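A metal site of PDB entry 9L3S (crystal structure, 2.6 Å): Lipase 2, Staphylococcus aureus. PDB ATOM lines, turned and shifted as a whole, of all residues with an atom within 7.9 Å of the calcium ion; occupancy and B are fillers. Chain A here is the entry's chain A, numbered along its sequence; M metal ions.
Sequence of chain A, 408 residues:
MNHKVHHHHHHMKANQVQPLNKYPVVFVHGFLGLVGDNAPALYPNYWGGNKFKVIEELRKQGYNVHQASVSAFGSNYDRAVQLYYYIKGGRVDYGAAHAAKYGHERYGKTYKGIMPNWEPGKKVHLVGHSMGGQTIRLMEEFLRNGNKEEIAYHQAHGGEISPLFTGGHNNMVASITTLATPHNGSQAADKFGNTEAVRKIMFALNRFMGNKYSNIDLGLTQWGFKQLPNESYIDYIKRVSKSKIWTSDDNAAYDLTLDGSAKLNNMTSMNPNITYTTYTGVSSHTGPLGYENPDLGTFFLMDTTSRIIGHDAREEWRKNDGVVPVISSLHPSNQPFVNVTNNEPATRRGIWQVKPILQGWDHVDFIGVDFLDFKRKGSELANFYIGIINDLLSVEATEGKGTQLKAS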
ATOM      1  N   LYS A  51       5.345 -23.029  28.009  1.00  0.00           N
ATOM      2  CA  LYS A  51       5.005 -22.824  26.621  1.00  0.00           C
ATOM      3  C   LYS A  51       4.463 -24.109  25.995  1.00  0.00           C
ATOM      4  O   LYS A  51       3.517 -24.044  25.205  1.00  0.00           O
ATOM      5  CB  LYS A  51       6.182 -22.260  25.828  1.00  0.00           C
ATOM      6  CG  LYS A  51       6.790 -20.985  26.414  1.00  0.00           C
ATOM      7  CD  LYS A  51       7.606 -20.177  25.432  1.00  0.00           C
ATOM      8  CE  LYS A  51       8.153 -18.945  26.126  1.00  0.00           C
ATOM      9  NZ  LYS A  51       8.793 -18.050  25.144  1.00  0.00           N
ATOM     10  N   SER A 283      21.176 -16.327  18.084  1.00  0.00           N
ATOM     11  CA  SER A 283      20.489 -15.369  18.922  1.00  0.00           C
ATOM     12  C   SER A 283      21.457 -14.232  19.221  1.00  0.00           C
ATOM     13  O   SER A 283      21.336 -13.521  20.224  1.00  0.00           O
ATOM     14  CB  SER A 283      19.992 -16.045  20.181  1.00  0.00           C
ATOM     15  OG  SER A 283      19.471 -15.109  21.108  1.00  0.00           O
ATOM     16  N   ASP A 295      21.115 -10.669  20.913  1.00  0.00           N
ATOM     17  CA  ASP A 295      19.856 -10.017  20.584  1.00  0.00           C
ATOM     18  C   ASP A 295      19.088  -9.746  21.869  1.00  0.00           C
ATOM     19  O   ASP A 295      19.132 -10.564  22.796  1.00  0.00           O
ATOM     20  CB  ASP A 295      18.958 -10.963  19.780  1.00  0.00           C
ATOM     21  CG  ASP A 295      19.517 -11.451  18.447  1.00  0.00           C
ATOM     22  OD1 ASP A 295      20.465 -10.815  17.928  1.00  0.00           O
ATOM     23  OD2 ASP A 295      18.996 -12.472  17.933  1.00  0.00           O
ATOM     24  N   LEU A 296      18.371  -8.610  21.934  1.00  0.00           N
ATOM     25  CA  LEU A 296      17.271  -8.525  22.880  1.00  0.00           C
ATOM     26  C   LEU A 296      16.431  -9.775  22.622  1.00  0.00           C
ATOM     27  O   LEU A 296      16.174 -10.125  21.459  1.00  0.00           O
ATOM     28  CB  LEU A 296      16.446  -7.247  22.631  1.00  0.00           C
ATOM     29  CG  LEU A 296      16.389  -6.192  23.748  1.00  0.00           C
ATOM     30  CD1 LEU A 296      15.123  -6.303  24.569  1.00  0.00           C
ATOM     31  CD2 LEU A 296      17.594  -6.261  24.671  1.00  0.00           C
ATOM     32  N   GLY A 297      16.104 -10.497  23.689  1.00  0.00           N
ATOM     33  CA  GLY A 297      15.343 -11.714  23.461  1.00  0.00           C
ATOM     34  C   GLY A 297      16.134 -12.963  23.836  1.00  0.00           C
ATOM     35  O   GLY A 297      15.555 -13.992  24.171  1.00  0.00           O
ATOM     36  N   THR A 298      17.462 -12.830  23.779  1.00  0.00           N
ATOM     37  CA  THR A 298      18.341 -13.766  24.438  1.00  0.00           C
ATOM     38  C   THR A 298      18.036 -13.729  25.924  1.00  0.00           C
ATOM     39  O   THR A 298      18.255 -12.711  26.575  1.00  0.00           O
ATOM     40  CB  THR A 298      19.811 -13.364  24.268  1.00  0.00           C
ATOM     41  OG1 THR A 298      20.042 -12.925  22.921  1.00  0.00           O
ATOM     42  CG2 THR A 298      20.751 -14.487  24.589  1.00  0.00           C
ATOM     43  N   PHE A 299      17.522 -14.834  26.471  1.00  0.00           N
ATOM     44  CA  PHE A 299      17.311 -14.953  27.897  1.00  0.00           C
ATOM     45  C   PHE A 299      18.475 -14.317  28.669  1.00  0.00           C
ATOM     46  O   PHE A 299      19.638 -14.552  28.360  1.00  0.00           O
ATOM     47  CB  PHE A 299      17.103 -16.417  28.274  1.00  0.00           C
ATOM     48  CG  PHE A 299      16.661 -16.617  29.694  1.00  0.00           C
ATOM     49  CD1 PHE A 299      15.379 -16.274  30.086  1.00  0.00           C
ATOM     50  CD2 PHE A 299      17.536 -17.117  30.636  1.00  0.00           C
ATOM     51  CE1 PHE A 299      14.978 -16.441  31.399  1.00  0.00           C
ATOM     52  CE2 PHE A 299      17.139 -17.281  31.961  1.00  0.00           C
ATOM     53  CZ  PHE A 299      15.862 -16.948  32.331  1.00  0.00           C
ATOM     54  N   PHE A 300      18.154 -13.510  29.686  1.00  0.00           N
ATOM     55  CA  PHE A 300      19.048 -12.490  30.215  1.00  0.00           C
ATOM     56  C   PHE A 300      20.230 -13.110  30.974  1.00  0.00           C
ATOM     57  O   PHE A 300      21.278 -12.478  31.085  1.00  0.00           O
ATOM     58  CB  PHE A 300      18.297 -11.498  31.111  1.00  0.00           C
ATOM     59  CG  PHE A 300      17.837 -12.107  32.423  1.00  0.00           C
ATOM     60  CD1 PHE A 300      16.710 -12.927  32.459  1.00  0.00           C
ATOM     61  CD2 PHE A 300      18.556 -11.903  33.586  1.00  0.00           C
ATOM     62  CE1 PHE A 300      16.314 -13.526  33.645  1.00  0.00           C
ATOM     63  CE2 PHE A 300      18.159 -12.502  34.771  1.00  0.00           C
ATOM     64  CZ  PHE A 300      17.053 -13.323  34.794  1.00  0.00           C
ATOM     65  N   MET A 302      22.042 -15.392  30.026  1.00  0.00           N
ATOM     66  CA  MET A 302      23.079 -15.716  29.067  1.00  0.00           C
ATOM     67  C   MET A 302      23.694 -14.454  28.454  1.00  0.00           C
ATOM     68  O   MET A 302      24.416 -14.529  27.471  1.00  0.00           O
ATOM     69  CB  MET A 302      22.502 -16.571  27.955  1.00  0.00           C
ATOM     70  CG  MET A 302      22.389 -17.984  28.361  1.00  0.00           C
ATOM     71  SD  MET A 302      21.583 -18.910  27.046  1.00  0.00           S
ATOM     72  CE  MET A 302      20.078 -17.992  26.782  1.00  0.00           C
ATOM     73  N   ASP A 321      24.088 -18.941  20.565  1.00  0.00           N
ATOM     74  CA  ASP A 321      22.702 -18.963  21.010  1.00  0.00           C
ATOM     75  C   ASP A 321      22.586 -18.437  22.441  1.00  0.00           C
ATOM     76  O   ASP A 321      21.554 -18.627  23.079  1.00  0.00           O
ATOM     77  CB  ASP A 321      22.114 -20.379  20.990  1.00  0.00           C
ATOM     78  CG  ASP A 321      22.726 -21.376  21.965  1.00  0.00           C
ATOM     79  OD1 ASP A 321      23.542 -20.940  22.832  1.00  0.00           O
ATOM     80  OD2 ASP A 321      22.391 -22.586  21.855  1.00  0.00           O
ATOM     81  N   GLY A 360      17.015 -16.742  15.734  1.00  0.00           N
ATOM     82  CA  GLY A 360      16.439 -16.072  16.889  1.00  0.00           C
ATOM     83  C   GLY A 360      15.962 -17.001  18.000  1.00  0.00           C
ATOM     84  O   GLY A 360      15.219 -16.574  18.897  1.00  0.00           O
ATOM     85  N   TRP A 361      16.358 -18.279  17.944  1.00  0.00           N
ATOM     86  CA  TRP A 361      16.213 -19.162  19.097  1.00  0.00           C
ATOM     87  C   TRP A 361      17.479 -19.120  19.937  1.00  0.00           C
ATOM     88  O   TRP A 361      18.566 -19.263  19.395  1.00  0.00           O
ATOM     89  CB  TRP A 361      15.963 -20.593  18.642  1.00  0.00           C
ATOM     90  CG  TRP A 361      14.590 -20.804  18.074  1.00  0.00           C
ATOM     91  CD1 TRP A 361      13.934 -20.013  17.179  1.00  0.00           C
ATOM     92  CD2 TRP A 361      13.750 -21.955  18.315  1.00  0.00           C
ATOM     93  NE1 TRP A 361      12.724 -20.587  16.867  1.00  0.00           N
ATOM     94  CE2 TRP A 361      12.591 -21.779  17.547  1.00  0.00           C
ATOM     95  CE3 TRP A 361      13.877 -23.106  19.104  1.00  0.00           C
ATOM     96  CZ2 TRP A 361      11.554 -22.699  17.544  1.00  0.00           C
ATOM     97  CZ3 TRP A 361      12.853 -24.030  19.084  1.00  0.00           C
ATOM     98  CH2 TRP A 361      11.709 -23.834  18.315  1.00  0.00           C
ATOM     99  N   ASP A 362      17.340 -18.927  21.241  1.00  0.00           N
ATOM    100  CA  ASP A 362      18.480 -18.953  22.123  1.00  0.00           C
ATOM    101  C   ASP A 362      18.566 -20.321  22.791  1.00  0.00           C
ATOM    102  O   ASP A 362      17.695 -21.187  22.616  1.00  0.00           O
ATOM    103  CB  ASP A 362      18.488 -17.772  23.086  1.00  0.00           C
ATOM    104  CG  ASP A 362      17.427 -17.802  24.168  1.00  0.00           C
ATOM    105  OD1 ASP A 362      16.912 -18.911  24.491  1.00  0.00           O
ATOM    106  OD2 ASP A 362      17.086 -16.705  24.674  1.00  0.00           O
ATOM    107  N   HIS A 363      19.625 -20.518  23.578  1.00  0.00           N
ATOM    108  CA  HIS A 363      19.896 -21.797  24.190  1.00  0.00           C
ATOM    109  C   HIS A 363      18.627 -22.357  24.799  1.00  0.00           C
ATOM    110  O   HIS A 363      18.316 -23.521  24.599  1.00  0.00           O
ATOM    111  CB  HIS A 363      20.939 -21.668  25.298  1.00  0.00           C
ATOM    112  CG  HIS A 363      21.535 -22.990  25.617  1.00  0.00           C
ATOM    113  ND1 HIS A 363      22.373 -23.638  24.746  1.00  0.00           N
ATOM    114  CD2 HIS A 363      21.379 -23.801  26.670  1.00  0.00           C
ATOM    115  CE1 HIS A 363      22.720 -24.797  25.283  1.00  0.00           C
ATOM    116  NE2 HIS A 363      22.142 -24.915  26.452  1.00  0.00           N
ATOM    117  N   VAL A 364      17.907 -21.509  25.554  1.00  0.00           N
ATOM    118  CA  VAL A 364      16.814 -21.992  26.390  1.00  0.00           C
ATOM    119  C   VAL A 364      15.484 -21.932  25.633  1.00  0.00           C
ATOM    120  O   VAL A 364      14.522 -22.566  26.059  1.00  0.00           O
ATOM    121  CB  VAL A 364      16.767 -21.304  27.764  1.00  0.00           C
ATOM    122  CG1 VAL A 364      18.075 -21.501  28.514  1.00  0.00           C
ATOM    123  CG2 VAL A 364      16.460 -19.821  27.659  1.00  0.00           C
ATOM    124  N   ASP A 365      15.445 -21.217  24.498  1.00  0.00           N
ATOM    125  CA  ASP A 365      14.221 -21.201  23.711  1.00  0.00           C
ATOM    126  C   ASP A 365      13.815 -22.625  23.323  1.00  0.00           C
ATOM    127  O   ASP A 365      12.638 -22.928  23.230  1.00  0.00           O
ATOM    128  CB  ASP A 365      14.259 -20.159  22.591  1.00  0.00           C
ATOM    129  CG  ASP A 365      14.174 -18.728  23.103  1.00  0.00           C
ATOM    130  OD1 ASP A 365      13.312 -18.447  23.972  1.00  0.00           O
ATOM    131  OD2 ASP A 365      14.952 -17.899  22.631  1.00  0.00           O
ATOM    132  N   PHE A 366      14.793 -23.506  23.171  1.00  0.00           N
ATOM    133  CA  PHE A 366      14.529 -24.876  22.723  1.00  0.00           C
ATOM    134  C   PHE A 366      13.703 -25.644  23.754  1.00  0.00           C
ATOM    135  O   PHE A 366      13.109 -26.668  23.419  1.00  0.00           O
ATOM    136  CB  PHE A 366      15.849 -25.628  22.512  1.00  0.00           C
ATOM    137  CG  PHE A 366      16.487 -25.309  21.191  1.00  0.00           C
ATOM    138  CD1 PHE A 366      16.041 -25.945  20.038  1.00  0.00           C
ATOM    139  CD2 PHE A 366      17.483 -24.344  21.086  1.00  0.00           C
ATOM    140  CE1 PHE A 366      16.599 -25.634  18.803  1.00  0.00           C
ATOM    141  CE2 PHE A 366      18.046 -24.042  19.851  1.00  0.00           C
ATOM    142  CZ  PHE A 366      17.600 -24.689  18.707  1.00  0.00           C
ATOM    143  N   VAL A 369      11.643 -22.012  28.244  1.00  0.00           N
ATOM    144  CA  VAL A 369      11.657 -21.484  29.599  1.00  0.00           C
ATOM    145  C   VAL A 369      11.977 -19.998  29.597  1.00  0.00           C
ATOM    146  O   VAL A 369      12.030 -19.408  30.659  1.00  0.00           O
ATOM    147  CB  VAL A 369      12.596 -22.257  30.540  1.00  0.00           C
ATOM    148  CG1 VAL A 369      12.259 -23.740  30.547  1.00  0.00           C
ATOM    149  CG2 VAL A 369      14.054 -22.046  30.191  1.00  0.00           C
ATOM    150  N   ASP A 370      12.152 -19.395  28.417  1.00  0.00           N
ATOM    151  CA  ASP A 370      12.369 -17.956  28.327  1.00  0.00           C
ATOM    152  C   ASP A 370      11.003 -17.266  28.316  1.00  0.00           C
ATOM    153  O   ASP A 370      10.531 -16.855  27.261  1.00  0.00           O
ATOM    154  CB  ASP A 370      13.302 -17.610  27.160  1.00  0.00           C
ATOM    155  CG  ASP A 370      13.633 -16.145  26.881  1.00  0.00           C
ATOM    156  OD1 ASP A 370      13.185 -15.274  27.647  1.00  0.00           O
ATOM    157  OD2 ASP A 370      14.320 -15.886  25.878  1.00  0.00           O
ATOM    158  N   PHE A 371      10.381 -17.134  29.499  1.00  0.00           N
ATOM    159  CA  PHE A 371       9.052 -16.537  29.583  1.00  0.00           C
ATOM    160  C   PHE A 371       9.098 -15.046  29.243  1.00  0.00           C
ATOM    161  O   PHE A 371       8.058 -14.467  28.958  1.00  0.00           O
ATOM    162  CB  PHE A 371       8.476 -16.707  30.986  1.00  0.00           C
ATOM    163  CG  PHE A 371       9.333 -16.087  32.055  1.00  0.00           C
ATOM    164  CD1 PHE A 371       9.228 -14.738  32.363  1.00  0.00           C
ATOM    165  CD2 PHE A 371      10.260 -16.859  32.738  1.00  0.00           C
ATOM    166  CE1 PHE A 371      10.019 -14.178  33.358  1.00  0.00           C
ATOM    167  CE2 PHE A 371      11.063 -16.292  33.728  1.00  0.00           C
ATOM    168  CZ  PHE A 371      10.943 -14.952  34.027  1.00  0.00           C
ATOM    169  N   LEU A 372      10.295 -14.438  29.246  1.00  0.00           N
ATOM    170  CA  LEU A 372      10.451 -13.059  28.817  1.00  0.00           C
ATOM    171  C   LEU A 372      10.289 -12.884  27.299  1.00  0.00           C
ATOM    172  O   LEU A 372      10.138 -11.753  26.850  1.00  0.00           O
ATOM    173  CB  LEU A 372      11.808 -12.505  29.276  1.00  0.00           C
ATOM    174  CG  LEU A 372      12.027 -12.057  30.733  1.00  0.00           C
ATOM    175  CD1 LEU A 372      10.741 -11.929  31.510  1.00  0.00           C
ATOM    176  CD2 LEU A 372      13.017 -12.942  31.485  1.00  0.00           C
ATOM    177  N   ASP A 373      10.314 -13.953  26.486  1.00  0.00           N
ATOM    178  CA  ASP A 373      10.412 -13.805  25.029  1.00  0.00           C
ATOM    179  C   ASP A 373       9.078 -14.156  24.347  1.00  0.00           C
ATOM    180  O   ASP A 373       8.824 -15.314  24.016  1.00  0.00           O
ATOM    181  CB  ASP A 373      11.623 -14.565  24.470  1.00  0.00           C
ATOM    182  CG  ASP A 373      11.909 -14.361  22.984  1.00  0.00           C
ATOM    183  OD1 ASP A 373      11.092 -13.699  22.302  1.00  0.00           O
ATOM    184  OD2 ASP A 373      12.959 -14.842  22.506  1.00  0.00           O
ATOM    185  N   PHE A 374       8.249 -13.131  24.084  1.00  0.00           N
ATOM    186  CA  PHE A 374       6.923 -13.260  23.488  1.00  0.00           C
ATOM    187  C   PHE A 374       7.052 -13.757  22.047  1.00  0.00           C
ATOM    188  O   PHE A 374       6.146 -14.418  21.546  1.00  0.00           O
ATOM    189  CB  PHE A 374       6.150 -11.927  23.528  1.00  0.00           C
ATOM    190  CG  PHE A 374       6.349 -11.106  24.782  1.00  0.00           C
ATOM    191  CD1 PHE A 374       6.239 -11.684  26.050  1.00  0.00           C
ATOM    192  CD2 PHE A 374       6.679  -9.753  24.711  1.00  0.00           C
ATOM    193  CE1 PHE A 374       6.443 -10.930  27.203  1.00  0.00           C
ATOM    194  CE2 PHE A 374       6.888  -9.007  25.864  1.00  0.00           C
ATOM    195  CZ  PHE A 374       6.773  -9.588  27.118  1.00  0.00           C
ATOM    196  N   LYS A 375       8.182 -13.456  21.398  1.00  0.00           N
ATOM    197  CA  LYS A 375       8.419 -13.813  20.012  1.00  0.00           C
ATOM    198  C   LYS A 375       8.477 -15.333  19.846  1.00  0.00           C
ATOM    199  O   LYS A 375       8.259 -15.844  18.752  1.00  0.00           O
ATOM    200  CB  LYS A 375       9.633 -13.067  19.430  1.00  0.00           C
ATOM    201  CG  LYS A 375       9.523 -11.543  19.386  1.00  0.00           C
ATOM    202  CD  LYS A 375      10.043 -10.809  18.116  1.00  0.00           C
ATOM    203  CE  LYS A 375      11.454 -10.254  18.177  1.00  0.00           C
ATOM    204  NZ  LYS A 375      12.489 -11.316  18.286  1.00  0.00           N
ATOM    205  N   ARG A 376       8.721 -16.063  20.944  1.00  0.00           N
ATOM    206  CA  ARG A 376       8.839 -17.503  20.866  1.00  0.00           C
ATOM    207  C   ARG A 376       7.570 -18.167  21.420  1.00  0.00           C
ATOM    208  O   ARG A 376       7.485 -18.459  22.606  1.00  0.00           O
ATOM    209  CB  ARG A 376      10.061 -17.942  21.670  1.00  0.00           C
ATOM    210  CG  ARG A 376      11.394 -17.460  21.115  1.00  0.00           C
ATOM    211  CD  ARG A 376      11.892 -18.433  20.060  1.00  0.00           C
ATOM    212  NE  ARG A 376      11.238 -18.330  18.770  1.00  0.00           N
ATOM    213  CZ  ARG A 376      11.384 -17.281  17.954  1.00  0.00           C
ATOM    214  NH1 ARG A 376      10.818 -17.299  16.764  1.00  0.00           N
ATOM    215  NH2 ARG A 376      12.124 -16.245  18.333  1.00  0.00           N
HETATM  216 CA    CA M   1      14.959 -15.979  23.590  1.00  0.00          CA
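The backbone NH (N) of Phe 299 sits close to the side-chain carboxylate (OD2) of Asp 370 (3.4 Å). The backbone carbonyl oxygen (O) of Asp 370 sits at hydrogen-bond distance from the side-chain amino group (NZ) of Lys 51 (3.0 Å). N of Leu 372 sits close to OD1 of Asp 370 (3.4 Å). The side-chain carboxylate of Asp 362 sits close to the backbone NH of Phe 299, at 2.6 Å. N of Val 364 lies within hydrogen-bond range of OD1 of Asp 362 (3.0 Å). The backbone carbonyl oxygen (O) of Asp 373 lies within hydrogen-bond range of the side-chain amino group (NZ) of Lys 51 (3.0 Å). The backbone NH of Lys 375 lies within hydrogen-bond range of the side-chain carboxylate of Asp 373 (3.1 Å).
The calcium ion is bound by OD2 of Asp 365 (2.1 Å), O of Gly 297 (2.2 Å), OD2 of Asp 370 (2.4 Å), OD2 of Asp 362 (2.5 Å) and OD2 of Asp 373 (2.5 Å). Slightly farther from the calcium ion lies OD1 of Asp 365 (3.0 Å).
Of the 25 residues printed, 5 come within 4 Å of the calcium ion.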
